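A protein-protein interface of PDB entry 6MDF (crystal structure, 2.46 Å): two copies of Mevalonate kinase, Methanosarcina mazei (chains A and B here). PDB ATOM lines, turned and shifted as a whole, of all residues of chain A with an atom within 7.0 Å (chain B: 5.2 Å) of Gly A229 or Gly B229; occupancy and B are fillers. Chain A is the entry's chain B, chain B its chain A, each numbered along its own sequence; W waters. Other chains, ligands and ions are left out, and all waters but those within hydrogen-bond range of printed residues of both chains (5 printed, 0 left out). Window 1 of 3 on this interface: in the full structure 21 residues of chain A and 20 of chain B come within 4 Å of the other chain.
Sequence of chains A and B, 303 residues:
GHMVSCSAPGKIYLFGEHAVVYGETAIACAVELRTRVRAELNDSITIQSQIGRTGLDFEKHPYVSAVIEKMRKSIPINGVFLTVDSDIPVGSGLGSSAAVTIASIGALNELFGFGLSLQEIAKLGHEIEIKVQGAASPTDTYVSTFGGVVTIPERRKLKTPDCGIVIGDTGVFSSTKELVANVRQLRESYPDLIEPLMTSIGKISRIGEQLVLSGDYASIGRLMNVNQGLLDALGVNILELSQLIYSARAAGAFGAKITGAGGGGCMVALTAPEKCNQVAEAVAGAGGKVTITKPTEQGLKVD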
ATOM      1  N   MET A 224      12.867  22.011  17.085  1.00  0.00           N
ATOM      2  CA  MET A 224      13.312  21.009  18.045  1.00  0.00           C
ATOM      3  C   MET A 224      14.354  21.592  18.993  1.00  0.00           C
ATOM      4  O   MET A 224      14.318  21.328  20.200  1.00  0.00           O
ATOM      5  CB  MET A 224      13.863  19.784  17.310  1.00  0.00           C
ATOM      6  CG  MET A 224      12.794  18.916  16.650  1.00  0.00           C
ATOM      7  SD  MET A 224      13.442  17.658  15.517  1.00  0.00           S
ATOM      8  CE  MET A 224      14.525  16.723  16.589  1.00  0.00           C
ATOM      9  N   ASN A 225      15.283  22.396  18.465  1.00  0.00           N
ATOM     10  CA  ASN A 225      16.301  23.008  19.314  1.00  0.00           C
ATOM     11  C   ASN A 225      15.675  23.954  20.332  1.00  0.00           C
ATOM     12  O   ASN A 225      16.121  24.023  21.483  1.00  0.00           O
ATOM     13  CB  ASN A 225      17.328  23.752  18.461  1.00  0.00           C
ATOM     14  CG  ASN A 225      18.030  22.850  17.464  1.00  0.00           C
ATOM     15  OD1 ASN A 225      18.108  21.631  17.647  1.00  0.00           O
ATOM     16  ND2 ASN A 225      18.555  23.448  16.401  1.00  0.00           N
ATOM     17  N   VAL A 226      14.645  24.698  19.923  1.00  0.00           N
ATOM     18  CA  VAL A 226      13.908  25.534  20.868  1.00  0.00           C
ATOM     19  C   VAL A 226      13.248  24.668  21.934  1.00  0.00           C
ATOM     20  O   VAL A 226      13.361  24.934  23.136  1.00  0.00           O
ATOM     21  CB  VAL A 226      12.870  26.398  20.130  1.00  0.00           C
ATOM     22  CG1 VAL A 226      12.117  27.280  21.121  1.00  0.00           C
ATOM     23  CG2 VAL A 226      13.536  27.232  19.052  1.00  0.00           C
ATOM     24  N   ASN A 227      12.549  23.614  21.503  1.00  0.00           N
ATOM     25  CA  ASN A 227      11.902  22.711  22.448  1.00  0.00           C
ATOM     26  C   ASN A 227      12.900  22.164  23.460  1.00  0.00           C
ATOM     27  O   ASN A 227      12.586  22.053  24.652  1.00  0.00           O
ATOM     28  CB  ASN A 227      11.219  21.568  21.690  1.00  0.00           C
ATOM     29  CG  ASN A 227      10.033  20.979  22.448  1.00  0.00           C
ATOM     30  OD1 ASN A 227       9.115  20.422  21.841  1.00  0.00           O
ATOM     31  ND2 ASN A 227      10.052  21.092  23.771  1.00  0.00           N
ATOM     32  N   GLN A 228      14.115  21.833  23.008  1.00  0.00           N
ATOM     33  CA  GLN A 228      15.115  21.268  23.911  1.00  0.00           C
ATOM     34  C   GLN A 228      15.501  22.255  25.007  1.00  0.00           C
ATOM     35  O   GLN A 228      15.692  21.863  26.164  1.00  0.00           O
ATOM     36  CB  GLN A 228      16.351  20.833  23.123  1.00  0.00           C
ATOM     37  CG  GLN A 228      17.554  20.426  23.972  1.00  0.00           C
ATOM     38  CD  GLN A 228      17.252  19.305  24.961  1.00  0.00           C
ATOM     39  OE1 GLN A 228      16.324  18.518  24.770  1.00  0.00           O
ATOM     40  NE2 GLN A 228      18.057  19.218  26.016  1.00  0.00           N
ATOM     41  N   GLY A 229      15.621  23.539  24.662  1.00  0.00           N
ATOM     42  CA  GLY A 229      15.948  24.533  25.670  1.00  0.00           C
ATOM     43  C   GLY A 229      14.853  24.687  26.710  1.00  0.00           C
ATOM     44  O   GLY A 229      15.131  24.872  27.898  1.00  0.00           O
ATOM     45  N   LEU A 230      13.592  24.602  26.280  1.00  0.00           N
ATOM     46  CA  LEU A 230      12.488  24.663  27.231  1.00  0.00           C
ATOM     47  C   LEU A 230      12.523  23.480  28.192  1.00  0.00           C
ATOM     48  O   LEU A 230      12.348  23.652  29.403  1.00  0.00           O
ATOM     49  CB  LEU A 230      11.156  24.728  26.484  1.00  0.00           C
ATOM     50  CG  LEU A 230      11.003  25.954  25.576  1.00  0.00           C
ATOM     51  CD1 LEU A 230       9.596  26.051  25.001  1.00  0.00           C
ATOM     52  CD2 LEU A 230      11.359  27.226  26.327  1.00  0.00           C
ATOM     53  N   LEU A 231      12.757  22.273  27.674  1.00  0.00           N
ATOM     54  CA  LEU A 231      12.870  21.108  28.547  1.00  0.00           C
ATOM     55  C   LEU A 231      14.063  21.242  29.482  1.00  0.00           C
ATOM     56  O   LEU A 231      13.988  20.862  30.656  1.00  0.00           O
ATOM     57  CB  LEU A 231      12.979  19.831  27.712  1.00  0.00           C
ATOM     58  CG  LEU A 231      11.731  19.487  26.894  1.00  0.00           C
ATOM     59  CD1 LEU A 231      12.056  18.466  25.817  1.00  0.00           C
ATOM     60  CD2 LEU A 231      10.617  18.986  27.801  1.00  0.00           C
ATOM     61  N   ASP A 232      15.172  21.786  28.979  1.00  0.00           N
ATOM     62  CA  ASP A 232      16.314  22.061  29.842  1.00  0.00           C
ATOM     63  C   ASP A 232      15.940  23.054  30.933  1.00  0.00           C
ATOM     64  O   ASP A 232      16.417  22.948  32.069  1.00  0.00           O
ATOM     65  CB  ASP A 232      17.483  22.587  29.010  1.00  0.00           C
ATOM     66  CG  ASP A 232      18.714  22.871  29.845  1.00  0.00           C
ATOM     67  OD1 ASP A 232      18.764  23.938  30.494  1.00  0.00           O
ATOM     68  OD2 ASP A 232      19.636  22.030  29.850  1.00  0.00           O
ATOM     69  N   ALA A 233      15.082  24.025  30.604  1.00  0.00           N
ATOM     70  CA  ALA A 233      14.630  24.987  31.603  1.00  0.00           C
ATOM     71  C   ALA A 233      13.749  24.329  32.656  1.00  0.00           C
ATOM     72  O   ALA A 233      13.743  24.761  33.813  1.00  0.00           O
ATOM     73  CB  ALA A 233      13.883  26.136  30.926  1.00  0.00           C
ATOM     74  N   LEU A 234      13.009  23.287  32.282  1.00  0.00           N
ATOM     75  CA  LEU A 234      12.208  22.542  33.240  1.00  0.00           C
ATOM     76  C   LEU A 234      13.031  21.559  34.062  1.00  0.00           C
ATOM     77  O   LEU A 234      12.483  20.933  34.976  1.00  0.00           O
ATOM     78  CB  LEU A 234      11.082  21.801  32.517  1.00  0.00           C
ATOM     79  CG  LEU A 234      10.162  22.702  31.688  1.00  0.00           C
ATOM     80  CD1 LEU A 234       9.122  21.876  30.944  1.00  0.00           C
ATOM     81  CD2 LEU A 234       9.499  23.731  32.582  1.00  0.00           C
ATOM     82  N   GLY A 235      14.318  21.404  33.760  1.00  0.00           N
ATOM     83  CA  GLY A 235      15.209  20.607  34.578  1.00  0.00           C
ATOM     84  C   GLY A 235      15.326  19.145  34.209  1.00  0.00           C
ATOM     85  O   GLY A 235      15.874  18.372  35.006  1.00  0.00           O
ATOM     86  N   TYR A 246      24.413  18.315  21.196  1.00  0.00           N
ATOM     87  CA  TYR A 246      25.212  19.323  20.510  1.00  0.00           C
ATOM     88  C   TYR A 246      26.184  18.699  19.517  1.00  0.00           C
ATOM     89  O   TYR A 246      26.527  19.333  18.512  1.00  0.00           O
ATOM     90  CB  TYR A 246      25.942  20.199  21.530  1.00  0.00           C
ATOM     91  CG  TYR A 246      25.052  21.307  22.040  1.00  0.00           C
ATOM     92  CD1 TYR A 246      24.790  22.425  21.256  1.00  0.00           C
ATOM     93  CD2 TYR A 246      24.442  21.220  23.287  1.00  0.00           C
ATOM     94  CE1 TYR A 246      23.959  23.435  21.705  1.00  0.00           C
ATOM     95  CE2 TYR A 246      23.608  22.227  23.745  1.00  0.00           C
ATOM     96  CZ  TYR A 246      23.370  23.332  22.950  1.00  0.00           C
ATOM     97  OH  TYR A 246      22.543  24.335  23.400  1.00  0.00           O
ATOM     98  N   ARG A 249      24.099  18.267  16.405  1.00  0.00           N
ATOM     99  CA  ARG A 249      23.903  19.553  15.742  1.00  0.00           C
ATOM    100  C   ARG A 249      25.153  19.976  14.981  1.00  0.00           C
ATOM    101  O   ARG A 249      25.079  20.383  13.817  1.00  0.00           O
ATOM    102  CB  ARG A 249      23.515  20.618  16.771  1.00  0.00           C
ATOM    103  CG  ARG A 249      22.126  20.443  17.364  1.00  0.00           C
ATOM    104  CD  ARG A 249      21.897  21.399  18.528  1.00  0.00           C
ATOM    105  NE  ARG A 249      20.595  21.196  19.159  1.00  0.00           N
ATOM    106  CZ  ARG A 249      20.177  21.851  20.238  1.00  0.00           C
ATOM    107  NH1 ARG A 249      20.959  22.756  20.814  1.00  0.00           N
ATOM    108  NH2 ARG A 249      18.977  21.601  20.741  1.00  0.00           N
ATOM    109  N   ALA A 256      18.140  18.592  17.273  1.00  0.00           N
ATOM    110  CA  ALA A 256      18.355  17.523  18.236  1.00  0.00           C
ATOM    111  C   ALA A 256      17.740  17.931  19.566  1.00  0.00           C
ATOM    112  O   ALA A 256      17.792  19.103  19.948  1.00  0.00           O
ATOM    113  CB  ALA A 256      19.847  17.213  18.401  1.00  0.00           C
ATOM    114  N   LYS A 257      17.158  16.960  20.265  1.00  0.00           N
ATOM    115  CA  LYS A 257      16.462  17.242  21.513  1.00  0.00           C
ATOM    116  C   LYS A 257      16.252  15.945  22.281  1.00  0.00           C
ATOM    117  O   LYS A 257      16.367  14.846  21.731  1.00  0.00           O
ATOM    118  CB  LYS A 257      15.115  17.922  21.260  1.00  0.00           C
ATOM    119  CG  LYS A 257      14.148  17.075  20.452  1.00  0.00           C
ATOM    120  CD  LYS A 257      12.847  17.824  20.199  1.00  0.00           C
ATOM    121  CE  LYS A 257      11.917  17.777  21.403  1.00  0.00           C
ATOM    122  NZ  LYS A 257      11.308  16.432  21.567  1.00  0.00           N
ATOM    123  N   ASN B 225      19.209  28.383  36.664  1.00  0.00           N
ATOM    124  CA  ASN B 225      19.158  27.200  35.809  1.00  0.00           C
ATOM    125  C   ASN B 225      17.977  27.259  34.848  1.00  0.00           C
ATOM    126  O   ASN B 225      18.096  26.847  33.689  1.00  0.00           O
ATOM    127  CB  ASN B 225      19.099  25.935  36.663  1.00  0.00           C
ATOM    128  CG  ASN B 225      20.360  25.727  37.474  1.00  0.00           C
ATOM    129  OD1 ASN B 225      21.402  26.317  37.182  1.00  0.00           O
ATOM    130  ND2 ASN B 225      20.278  24.878  38.489  1.00  0.00           N
ATOM    131  N   VAL B 226      16.831  27.769  35.311  1.00  0.00           N
ATOM    132  CA  VAL B 226      15.708  27.999  34.405  1.00  0.00           C
ATOM    133  C   VAL B 226      16.088  29.017  33.341  1.00  0.00           C
ATOM    134  O   VAL B 226      15.761  28.853  32.159  1.00  0.00           O
ATOM    135  CB  VAL B 226      14.460  28.449  35.185  1.00  0.00           C
ATOM    136  CG1 VAL B 226      13.293  28.658  34.224  1.00  0.00           C
ATOM    137  CG2 VAL B 226      14.104  27.427  36.254  1.00  0.00           C
ATOM    138  N   ASN B 227      16.788  30.082  33.742  1.00  0.00           N
ATOM    139  CA  ASN B 227      17.235  31.077  32.775  1.00  0.00           C
ATOM    140  C   ASN B 227      18.172  30.467  31.743  1.00  0.00           C
ATOM    141  O   ASN B 227      18.147  30.862  30.572  1.00  0.00           O
ATOM    142  CB  ASN B 227      17.925  32.236  33.494  1.00  0.00           C
ATOM    143  CG  ASN B 227      17.830  33.546  32.729  1.00  0.00           C
ATOM    144  OD1 ASN B 227      17.909  34.623  33.318  1.00  0.00           O
ATOM    145  ND2 ASN B 227      17.657  33.463  31.416  1.00  0.00           N
ATOM    146  N   GLN B 228      18.997  29.502  32.151  1.00  0.00           N
ATOM    147  CA  GLN B 228      19.932  28.893  31.211  1.00  0.00           C
ATOM    148  C   GLN B 228      19.197  28.100  30.138  1.00  0.00           C
ATOM    149  O   GLN B 228      19.595  28.117  28.967  1.00  0.00           O
ATOM    150  CB  GLN B 228      20.929  28.007  31.958  1.00  0.00           C
ATOM    151  CG  GLN B 228      21.817  27.158  31.056  1.00  0.00           C
ATOM    152  CD  GLN B 228      22.633  27.979  30.069  1.00  0.00           C
ATOM    153  OE1 GLN B 228      22.856  29.178  30.266  1.00  0.00           O
ATOM    154  NE2 GLN B 228      23.098  27.328  29.007  1.00  0.00           N
ATOM    155  N   GLY B 229      18.118  27.409  30.514  1.00  0.00           N
ATOM    156  CA  GLY B 229      17.345  26.670  29.529  1.00  0.00           C
ATOM    157  C   GLY B 229      16.697  27.574  28.501  1.00  0.00           C
ATOM    158  O   GLY B 229      16.650  27.246  27.313  1.00  0.00           O
ATOM    159  N   LEU B 230      16.195  28.729  28.940  1.00  0.00           N
ATOM    160  CA  LEU B 230      15.616  29.686  28.004  1.00  0.00           C
ATOM    161  C   LEU B 230      16.680  30.264  27.079  1.00  0.00           C
ATOM    162  O   LEU B 230      16.443  30.422  25.875  1.00  0.00           O
ATOM    163  CB  LEU B 230      14.898  30.796  28.770  1.00  0.00           C
ATOM    164  CG  LEU B 230      13.721  30.331  29.632  1.00  0.00           C
ATOM    165  CD1 LEU B 230      13.071  31.498  30.352  1.00  0.00           C
ATOM    166  CD2 LEU B 230      12.706  29.599  28.775  1.00  0.00           C
ATOM    167  N   LEU B 231      17.860  30.577  27.623  1.00  0.00           N
ATOM    168  CA  LEU B 231      18.967  31.022  26.783  1.00  0.00           C
ATOM    169  C   LEU B 231      19.360  29.942  25.786  1.00  0.00           C
ATOM    170  O   LEU B 231      19.639  30.233  24.616  1.00  0.00           O
ATOM    171  CB  LEU B 231      20.165  31.401  27.651  1.00  0.00           C
ATOM    172  CG  LEU B 231      20.017  32.670  28.484  1.00  0.00           C
ATOM    173  CD1 LEU B 231      21.222  32.842  29.399  1.00  0.00           C
ATOM    174  CD2 LEU B 231      19.839  33.874  27.572  1.00  0.00           C
ATOM    175  N   ASP B 232      19.391  28.686  26.240  1.00  0.00           N
ATOM    176  CA  ASP B 232      19.615  27.566  25.333  1.00  0.00           C
ATOM    177  C   ASP B 232      18.529  27.504  24.267  1.00  0.00           C
ATOM    178  O   ASP B 232      18.816  27.240  23.095  1.00  0.00           O
ATOM    179  CB  ASP B 232      19.669  26.264  26.134  1.00  0.00           C
ATOM    180  CG  ASP B 232      20.089  25.073  25.296  1.00  0.00           C
ATOM    181  OD1 ASP B 232      19.248  24.538  24.547  1.00  0.00           O
ATOM    182  OD2 ASP B 232      21.265  24.672  25.390  1.00  0.00           O
ATOM    183  N   ALA B 233      17.276  27.758  24.657  1.00  0.00           N
ATOM    184  CA  ALA B 233      16.177  27.749  23.695  1.00  0.00           C
ATOM    185  C   ALA B 233      16.307  28.870  22.671  1.00  0.00           C
ATOM    186  O   ALA B 233      15.811  28.738  21.548  1.00  0.00           O
ATOM    187  CB  ALA B 233      14.839  27.856  24.427  1.00  0.00           C
ATOM    188  N   LEU B 234      16.960  29.975  23.034  1.00  0.00           N
ATOM    189  CA  LEU B 234      17.173  31.074  22.099  1.00  0.00           C
ATOM    190  C   LEU B 234      18.351  30.835  21.163  1.00  0.00           C
ATOM    191  O   LEU B 234      18.563  31.638  20.248  1.00  0.00           O
ATOM    192  CB  LEU B 234      17.377  32.385  22.863  1.00  0.00           C
ATOM    193  CG  LEU B 234      16.130  32.912  23.582  1.00  0.00           C
ATOM    194  CD1 LEU B 234      16.455  34.111  24.469  1.00  0.00           C
ATOM    195  CD2 LEU B 234      15.046  33.259  22.576  1.00  0.00           C
HETATM  196  O   HOH W   1      19.129  24.374  33.090  1.00  0.00           O
HETATM  197  O   HOH W   2      20.100  22.293  23.807  1.00  0.00           O
HETATM  198  O   HOH W   3      18.837  24.147  22.162  1.00  0.00           O
HETATM  199  O   HOH W   4      21.613  27.162  22.060  1.00  0.00           O
HETATM  200  O   HOH W   5      21.842  22.826  27.666  1.00  0.00           O
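Of the 10 printed residues of chain B, 5 touch a printed residue of chain A.
Hydrophobic or aromatic side chains of chain B within 4 Å of the printed part of chain A: Val B226, Leu B230 and Ala B233.
Hydrophobic or aromatic side chains of chain A within 4 Å of the printed part of chain B: Val A226, Leu A230, Ala A233 and Tyr A246.
Among the printed residues, 10 pairs touch across the chains.
Among the printed residues, no Asp or Glu carboxylate lies within 4 Å of a Lys or Arg side-chain nitrogen of the other chain.
OD1 of Asp B232 lies close to OH of Tyr A246, 3.5 Å away.
The backbone carbonyl oxygen of Gly A229 lies close to the backbone carbonyl oxygen of Gly B229, 2.9 Å away.
Water W3 lies within hydrogen-bond range of the side-chain carboxylate (OD1) of Asp B232 (2.5 Å), the backbone carbonyl oxygen (O) of Asn A225 (2.8 Å) and the guanidinium group (NH1) of Arg A249 (2.9 Å).
Water W2 lies within hydrogen-bond range of the side-chain carboxylate of Asp B232 (2.5 Å), the guanidinium group of Arg A249 (3.1 Å) and the side-chain hydroxyl of Tyr A246 (3.2 Å).
Water W1 bridges OD1 of Asp A232 and O of Asn B225.
Water W4 bridges the backbone carbonyl oxygen of Asp B232 (3.0 Å) and the side-chain hydroxyl of Tyr A246 (3.3 Å).
Water W5 lies within hydrogen-bond range of the side-chain carboxylate of Asp B232 (3.0 Å) and the side-chain carboxylate of Asp A232 (3.2 Å).
O of Val A226 touches CB of Ala B233 (3.5 Å).
Gly A229 touches Asp B232.
Gly A229 touches Ala B233.
CD2 of Leu A230 touches CD2 of Leu B230 (3.7 Å).
N of Leu A230 touches CB of Ala B233, 3.9 Å away.
Asp A232 touches Gly B229 (OD1 to CA, 3.2 Å).
Val B226 touches Ala A233 (O to CB, 3.5 Å).
Gly B229 touches Ala A233.
Val A226 touches Ala B233, and with the chains exchanged Ala A233 touches Val B226.
Gly A229 touches Ala B233, and with the chains exchanged Ala A233 touches Gly B229.
Leu B230 touches its own counterpart, Leu A230.
Leu A230 touches Ala B233, but with the chains exchanged Ala A233 does not touch Leu B230 (4.002 Å).
Positions printed for both chains: 225, 226, 227, 228, 229, 230, 231, 232, 233 and 234.
Of chain B, only Gly B229, Asp B232 and Ala B233 come within 4 Å of Gly A229.
Of the printed residues of chain B, Asp A232 touches Gly B229.
Of the printed residues of chain A, Val B226 touches Ala A233.
The nearest residue of chain B that does not touch Gly A229 is Leu B230 (4.1 Å).
The nearest printed residue of chain A that does not touch Val B226 is Asp A232 (5.6 Å).
NH1 of Arg A249 lies close to OH of Tyr A246, 3.4 Å away.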
